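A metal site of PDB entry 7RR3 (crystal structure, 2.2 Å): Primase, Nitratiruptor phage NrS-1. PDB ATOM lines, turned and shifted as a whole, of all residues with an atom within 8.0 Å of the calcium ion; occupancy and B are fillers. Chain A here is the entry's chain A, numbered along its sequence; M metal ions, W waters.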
ATOM      1  N   GLN A  16     -10.550  10.721  -9.986  1.00  0.00           N
ATOM      2  CA  GLN A  16     -11.791  11.485  -9.852  1.00  0.00           C
ATOM      3  C   GLN A  16     -12.023  11.897  -8.406  1.00  0.00           C
ATOM      4  O   GLN A  16     -13.152  11.936  -7.926  1.00  0.00           O
ATOM      5  CB  GLN A  16     -12.975  10.671 -10.374  1.00  0.00           C
ATOM      6  CG  GLN A  16     -12.783  10.133 -11.779  1.00  0.00           C
ATOM      7  CD  GLN A  16     -13.907   9.206 -12.204  1.00  0.00           C
ATOM      8  OE1 GLN A  16     -14.899   9.044 -11.485  1.00  0.00           O
ATOM      9  NE2 GLN A  16     -13.764   8.588 -13.365  1.00  0.00           N
ATOM     10  N   PHE A  66     -15.449  11.895  -4.082  1.00  0.00           N
ATOM     11  CA  PHE A  66     -15.311  11.115  -5.314  1.00  0.00           C
ATOM     12  C   PHE A  66     -16.390  11.547  -6.292  1.00  0.00           C
ATOM     13  O   PHE A  66     -17.580  11.499  -5.955  1.00  0.00           O
ATOM     14  CB  PHE A  66     -15.399   9.615  -5.030  1.00  0.00           C
ATOM     15  CG  PHE A  66     -15.134   8.758  -6.236  1.00  0.00           C
ATOM     16  CD1 PHE A  66     -13.831   8.390  -6.559  1.00  0.00           C
ATOM     17  CD2 PHE A  66     -16.168   8.311  -7.043  1.00  0.00           C
ATOM     18  CE1 PHE A  66     -13.584   7.597  -7.671  1.00  0.00           C
ATOM     19  CE2 PHE A  66     -15.917   7.526  -8.144  1.00  0.00           C
ATOM     20  CZ  PHE A  66     -14.625   7.165  -8.460  1.00  0.00           C
ATOM     21  N   VAL A  67     -15.977  11.957  -7.488  1.00  0.00           N
ATOM     22  CA  VAL A  67     -16.898  12.481  -8.491  1.00  0.00           C
ATOM     23  C   VAL A  67     -17.456  11.323  -9.299  1.00  0.00           C
ATOM     24  O   VAL A  67     -16.709  10.507  -9.847  1.00  0.00           O
ATOM     25  CB  VAL A  67     -16.194  13.501  -9.399  1.00  0.00           C
ATOM     26  CG1 VAL A  67     -17.191  14.135 -10.359  1.00  0.00           C
ATOM     27  CG2 VAL A  67     -15.505  14.562  -8.570  1.00  0.00           C
ATOM     28  N   LEU A  68     -18.782  11.253  -9.382  1.00  0.00           N
ATOM     29  CA  LEU A  68     -19.468  10.250 -10.190  1.00  0.00           C
ATOM     30  C   LEU A  68     -19.584  10.741 -11.624  1.00  0.00           C
ATOM     31  O   LEU A  68     -20.079  11.849 -11.867  1.00  0.00           O
ATOM     32  CB  LEU A  68     -20.856   9.955  -9.614  1.00  0.00           C
ATOM     33  CG  LEU A  68     -20.953   9.770  -8.103  1.00  0.00           C
ATOM     34  CD1 LEU A  68     -22.401   9.903  -7.656  1.00  0.00           C
ATOM     35  CD2 LEU A  68     -20.374   8.438  -7.687  1.00  0.00           C
ATOM     36  N   THR A  69     -19.130   9.918 -12.561  1.00  0.00           N
ATOM     37  CA  THR A  69     -19.145  10.264 -13.975  1.00  0.00           C
ATOM     38  C   THR A  69     -20.005   9.268 -14.744  1.00  0.00           C
ATOM     39  O   THR A  69     -20.302   8.170 -14.274  1.00  0.00           O
ATOM     40  CB  THR A  69     -17.720  10.273 -14.563  1.00  0.00           C
ATOM     41  OG1 THR A  69     -17.263   8.928 -14.729  1.00  0.00           O
ATOM     42  CG2 THR A  69     -16.767  11.021 -13.642  1.00  0.00           C
ATOM     43  N   LYS A  70     -20.388   9.665 -15.965  1.00  0.00           N
ATOM     44  CA  LYS A  70     -21.162   8.801 -16.838  1.00  0.00           C
ATOM     45  C   LYS A  70     -20.373   7.600 -17.346  1.00  0.00           C
ATOM     46  O   LYS A  70     -20.944   6.761 -18.057  1.00  0.00           O
ATOM     47  CB  LYS A  70     -21.697   9.594 -18.029  1.00  0.00           C
ATOM     48  CG  LYS A  70     -22.656  10.699 -17.669  1.00  0.00           C
ATOM     49  CD  LYS A  70     -23.203  11.369 -18.920  1.00  0.00           C
ATOM     50  CE  LYS A  70     -23.784  12.730 -18.601  1.00  0.00           C
ATOM     51  NZ  LYS A  70     -25.220  12.631 -18.260  1.00  0.00           N
ATOM     52  N   SER A  71     -19.095   7.501 -17.011  1.00  0.00           N
ATOM     53  CA  SER A  71     -18.244   6.424 -17.501  1.00  0.00           C
ATOM     54  C   SER A  71     -17.849   5.418 -16.437  1.00  0.00           C
ATOM     55  O   SER A  71     -17.361   4.332 -16.783  1.00  0.00           O
ATOM     56  CB  SER A  71     -16.972   7.010 -18.135  1.00  0.00           C
ATOM     57  OG  SER A  71     -17.295   7.919 -19.177  1.00  0.00           O
ATOM     58  N   ASP A  72     -18.040   5.726 -15.154  1.00  0.00           N
ATOM     59  CA  ASP A  72     -17.815   4.769 -14.082  1.00  0.00           C
ATOM     60  C   ASP A  72     -19.144   4.310 -13.487  1.00  0.00           C
ATOM     61  O   ASP A  72     -20.117   5.078 -13.473  1.00  0.00           O
ATOM     62  CB  ASP A  72     -16.922   5.367 -12.982  1.00  0.00           C
ATOM     63  CG  ASP A  72     -17.620   6.461 -12.191  1.00  0.00           C
ATOM     64  OD1 ASP A  72     -17.525   7.640 -12.604  1.00  0.00           O
ATOM     65  OD2 ASP A  72     -18.254   6.145 -11.175  1.00  0.00           O
ATOM     66  N   PRO A  73     -19.227   3.071 -13.007  1.00  0.00           N
ATOM     67  CA  PRO A  73     -20.538   2.487 -12.695  1.00  0.00           C
ATOM     68  C   PRO A  73     -20.981   2.599 -11.239  1.00  0.00           C
ATOM     69  O   PRO A  73     -21.892   1.882 -10.818  1.00  0.00           O
ATOM     70  CB  PRO A  73     -20.332   1.018 -13.082  1.00  0.00           C
ATOM     71  CG  PRO A  73     -18.911   0.763 -12.660  1.00  0.00           C
ATOM     72  CD  PRO A  73     -18.155   2.068 -12.872  1.00  0.00           C
ATOM     73  N   PHE A  74     -20.365   3.495 -10.475  1.00  0.00           N
ATOM     74  CA  PHE A  74     -20.670   3.581  -9.050  1.00  0.00           C
ATOM     75  C   PHE A  74     -21.957   4.369  -8.811  1.00  0.00           C
ATOM     76  O   PHE A  74     -22.123   5.478  -9.345  1.00  0.00           O
ATOM     77  CB  PHE A  74     -19.495   4.211  -8.301  1.00  0.00           C
ATOM     78  CG  PHE A  74     -18.216   3.443  -8.436  1.00  0.00           C
ATOM     79  CD1 PHE A  74     -18.091   2.194  -7.852  1.00  0.00           C
ATOM     80  CD2 PHE A  74     -17.157   3.958  -9.151  1.00  0.00           C
ATOM     81  CE1 PHE A  74     -16.908   1.470  -7.979  1.00  0.00           C
ATOM     82  CE2 PHE A  74     -15.982   3.244  -9.283  1.00  0.00           C
ATOM     83  CZ  PHE A  74     -15.856   1.995  -8.699  1.00  0.00           C
ATOM     84  N   VAL A  75     -22.854   3.800  -8.016  1.00  0.00           N
ATOM     85  CA  VAL A  75     -24.131   4.413  -7.681  1.00  0.00           C
ATOM     86  C   VAL A  75     -24.075   4.894  -6.239  1.00  0.00           C
ATOM     87  O   VAL A  75     -23.739   4.125  -5.337  1.00  0.00           O
ATOM     88  CB  VAL A  75     -25.296   3.428  -7.898  1.00  0.00           C
ATOM     89  CG1 VAL A  75     -26.627   4.100  -7.579  1.00  0.00           C
ATOM     90  CG2 VAL A  75     -25.284   2.892  -9.321  1.00  0.00           C
ATOM     91  N   PHE A  76     -24.421   6.156  -6.037  1.00  0.00           N
ATOM     92  CA  PHE A  76     -24.388   6.782  -4.711  1.00  0.00           C
ATOM     93  C   PHE A  76     -25.803   6.804  -4.149  1.00  0.00           C
ATOM     94  O   PHE A  76     -26.657   7.546  -4.620  1.00  0.00           O
ATOM     95  CB  PHE A  76     -23.801   8.190  -4.812  1.00  0.00           C
ATOM     96  CG  PHE A  76     -23.923   8.993  -3.538  1.00  0.00           C
ATOM     97  CD1 PHE A  76     -23.676   8.418  -2.309  1.00  0.00           C
ATOM     98  CD2 PHE A  76     -24.274  10.329  -3.595  1.00  0.00           C
ATOM     99  CE1 PHE A  76     -23.781   9.161  -1.151  1.00  0.00           C
ATOM    100  CE2 PHE A  76     -24.374  11.085  -2.439  1.00  0.00           C
ATOM    101  CZ  PHE A  76     -24.133  10.498  -1.208  1.00  0.00           C
ATOM    102  N   VAL A 118     -23.003   1.278  -4.748  1.00  0.00           N
ATOM    103  CA  VAL A 118     -23.304   0.069  -5.499  1.00  0.00           C
ATOM    104  C   VAL A 118     -22.789   0.246  -6.918  1.00  0.00           C
ATOM    105  O   VAL A 118     -22.831   1.344  -7.473  1.00  0.00           O
ATOM    106  CB  VAL A 118     -24.814  -0.239  -5.505  1.00  0.00           C
ATOM    107  CG1 VAL A 118     -25.121  -1.514  -6.288  1.00  0.00           C
ATOM    108  CG2 VAL A 118     -25.340  -0.360  -4.070  1.00  0.00           C
ATOM    109  N   GLY A 120     -23.832  -0.530 -10.342  1.00  0.00           N
ATOM    110  CA  GLY A 120     -24.990  -0.962 -11.104  1.00  0.00           C
ATOM    111  C   GLY A 120     -25.641   0.143 -11.918  1.00  0.00           C
ATOM    112  O   GLY A 120     -24.962   1.061 -12.385  1.00  0.00           O
ATOM    113  N   LYS A 121     -26.958   0.056 -12.080  1.00  0.00           N
ATOM    114  CA  LYS A 121     -27.713   1.009 -12.878  1.00  0.00           C
ATOM    115  C   LYS A 121     -29.025   1.315 -12.166  1.00  0.00           C
ATOM    116  O   LYS A 121     -29.733   0.396 -11.752  1.00  0.00           O
ATOM    117  CB  LYS A 121     -27.976   0.456 -14.285  1.00  0.00           C
ATOM    118  CG  LYS A 121     -28.953   1.286 -15.106  1.00  0.00           C
ATOM    119  CD  LYS A 121     -28.334   2.604 -15.528  1.00  0.00           C
ATOM    120  CE  LYS A 121     -29.398   3.643 -15.818  1.00  0.00           C
ATOM    121  NZ  LYS A 121     -28.806   5.006 -15.941  1.00  0.00           N
ATOM    122  N   TYR A 141     -27.903   8.868  -7.017  1.00  0.00           N
ATOM    123  CA  TYR A 141     -27.164   9.614  -8.017  1.00  0.00           C
ATOM    124  C   TYR A 141     -26.207   8.693  -8.750  1.00  0.00           C
ATOM    125  O   TYR A 141     -25.607   7.797  -8.144  1.00  0.00           O
ATOM    126  CB  TYR A 141     -26.382  10.773  -7.386  1.00  0.00           C
ATOM    127  CG  TYR A 141     -27.260  11.794  -6.685  1.00  0.00           C
ATOM    128  CD1 TYR A 141     -28.077  12.643  -7.425  1.00  0.00           C
ATOM    129  CD2 TYR A 141     -27.274  11.899  -5.309  1.00  0.00           C
ATOM    130  CE1 TYR A 141     -28.881  13.573  -6.798  1.00  0.00           C
ATOM    131  CE2 TYR A 141     -28.067  12.826  -4.666  1.00  0.00           C
ATOM    132  CZ  TYR A 141     -28.872  13.659  -5.416  1.00  0.00           C
ATOM    133  OH  TYR A 141     -29.676  14.589  -4.789  1.00  0.00           O
ATOM    134  N   GLU A 142     -26.066   8.912 -10.057  1.00  0.00           N
ATOM    135  CA  GLU A 142     -25.210   8.111 -10.910  1.00  0.00           C
ATOM    136  C   GLU A 142     -24.071   8.894 -11.546  1.00  0.00           C
ATOM    137  O   GLU A 142     -23.008   8.317 -11.788  1.00  0.00           O
ATOM    138  CB  GLU A 142     -26.023   7.438 -12.026  1.00  0.00           C
ATOM    139  CG  GLU A 142     -26.481   6.031 -11.696  1.00  0.00           C
ATOM    140  CD  GLU A 142     -27.488   5.499 -12.702  1.00  0.00           C
ATOM    141  OE1 GLU A 142     -28.070   6.313 -13.453  1.00  0.00           O
ATOM    142  OE2 GLU A 142     -27.705   4.270 -12.746  1.00  0.00           O
ATOM    143  N   SER A 143     -24.267  10.179 -11.830  1.00  0.00           N
ATOM    144  CA  SER A 143     -23.241  10.995 -12.473  1.00  0.00           C
ATOM    145  C   SER A 143     -23.567  12.456 -12.215  1.00  0.00           C
ATOM    146  O   SER A 143     -24.534  12.787 -11.537  1.00  0.00           O
ATOM    147  CB  SER A 143     -23.140  10.689 -13.973  1.00  0.00           C
ATOM    148  OG  SER A 143     -24.366  10.985 -14.619  1.00  0.00           O
ATOM    149  N   GLY A 144     -22.739  13.338 -12.782  1.00  0.00           N
ATOM    150  CA  GLY A 144     -22.921  14.767 -12.608  1.00  0.00           C
ATOM    151  C   GLY A 144     -22.900  15.219 -11.161  1.00  0.00           C
ATOM    152  O   GLY A 144     -23.518  16.226 -10.817  1.00  0.00           O
ATOM    153  N   ARG A 145     -22.187  14.497 -10.310  1.00  0.00           N
ATOM    154  CA  ARG A 145     -22.204  14.755  -8.883  1.00  0.00           C
ATOM    155  C   ARG A 145     -21.001  14.094  -8.235  1.00  0.00           C
ATOM    156  O   ARG A 145     -20.409  13.164  -8.788  1.00  0.00           O
ATOM    157  CB  ARG A 145     -23.501  14.247  -8.243  1.00  0.00           C
ATOM    158  CG  ARG A 145     -23.914  14.973  -6.978  1.00  0.00           C
ATOM    159  CD  ARG A 145     -25.397  14.800  -6.703  1.00  0.00           C
ATOM    160  NE  ARG A 145     -26.204  15.656  -7.569  1.00  0.00           N
ATOM    161  CZ  ARG A 145     -27.167  16.452  -7.138  1.00  0.00           C
ATOM    162  NH1 ARG A 145     -27.478  16.535  -5.853  1.00  0.00           N
ATOM    163  NH2 ARG A 145     -27.830  17.192  -8.017  1.00  0.00           N
HETATM  164 CA    CA M   1     -21.807   6.642 -13.041  1.00  0.00          CA
HETATM  165  O   HOH W   1     -20.616   6.959 -10.921  1.00  0.00           O
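The side-chain amino group of Lys 121 lies within salt-bridge range of the side-chain carboxylate of Glu 142, at 2.9 Å. OD2 of Asp 72 sits close to N of Phe 74 (3.5 Å). The side-chain carboxylate (OD1) of Asp 72 sits close to the side-chain amide oxygen (OE1) of Gln 16, 3.2 Å away. N of Ser 71 sits close to OG1 of Thr 69 (3.3 Å). The side-chain carboxylate (OD1) of Asp 72 sits at hydrogen-bond distance from the side-chain hydroxyl (OG1) of Thr 69 (2.5 Å).
Merely in contact with the calcium ion: Phe 74. Four residues have an atom within 4 Å of the calcium ion: Thr 69, Asp 72, Phe 74 and Glu 142. Along chain A the residues within 4 Å of the calcium ion span positions 69 to 142.
The calcium ion is bound by O of Asp 72, O of Glu 142, water W1 and O of Thr 69.
Water W1 bridges the side-chain carboxylate of Asp 72 and the backbone carbonyl oxygen of Phe 74.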
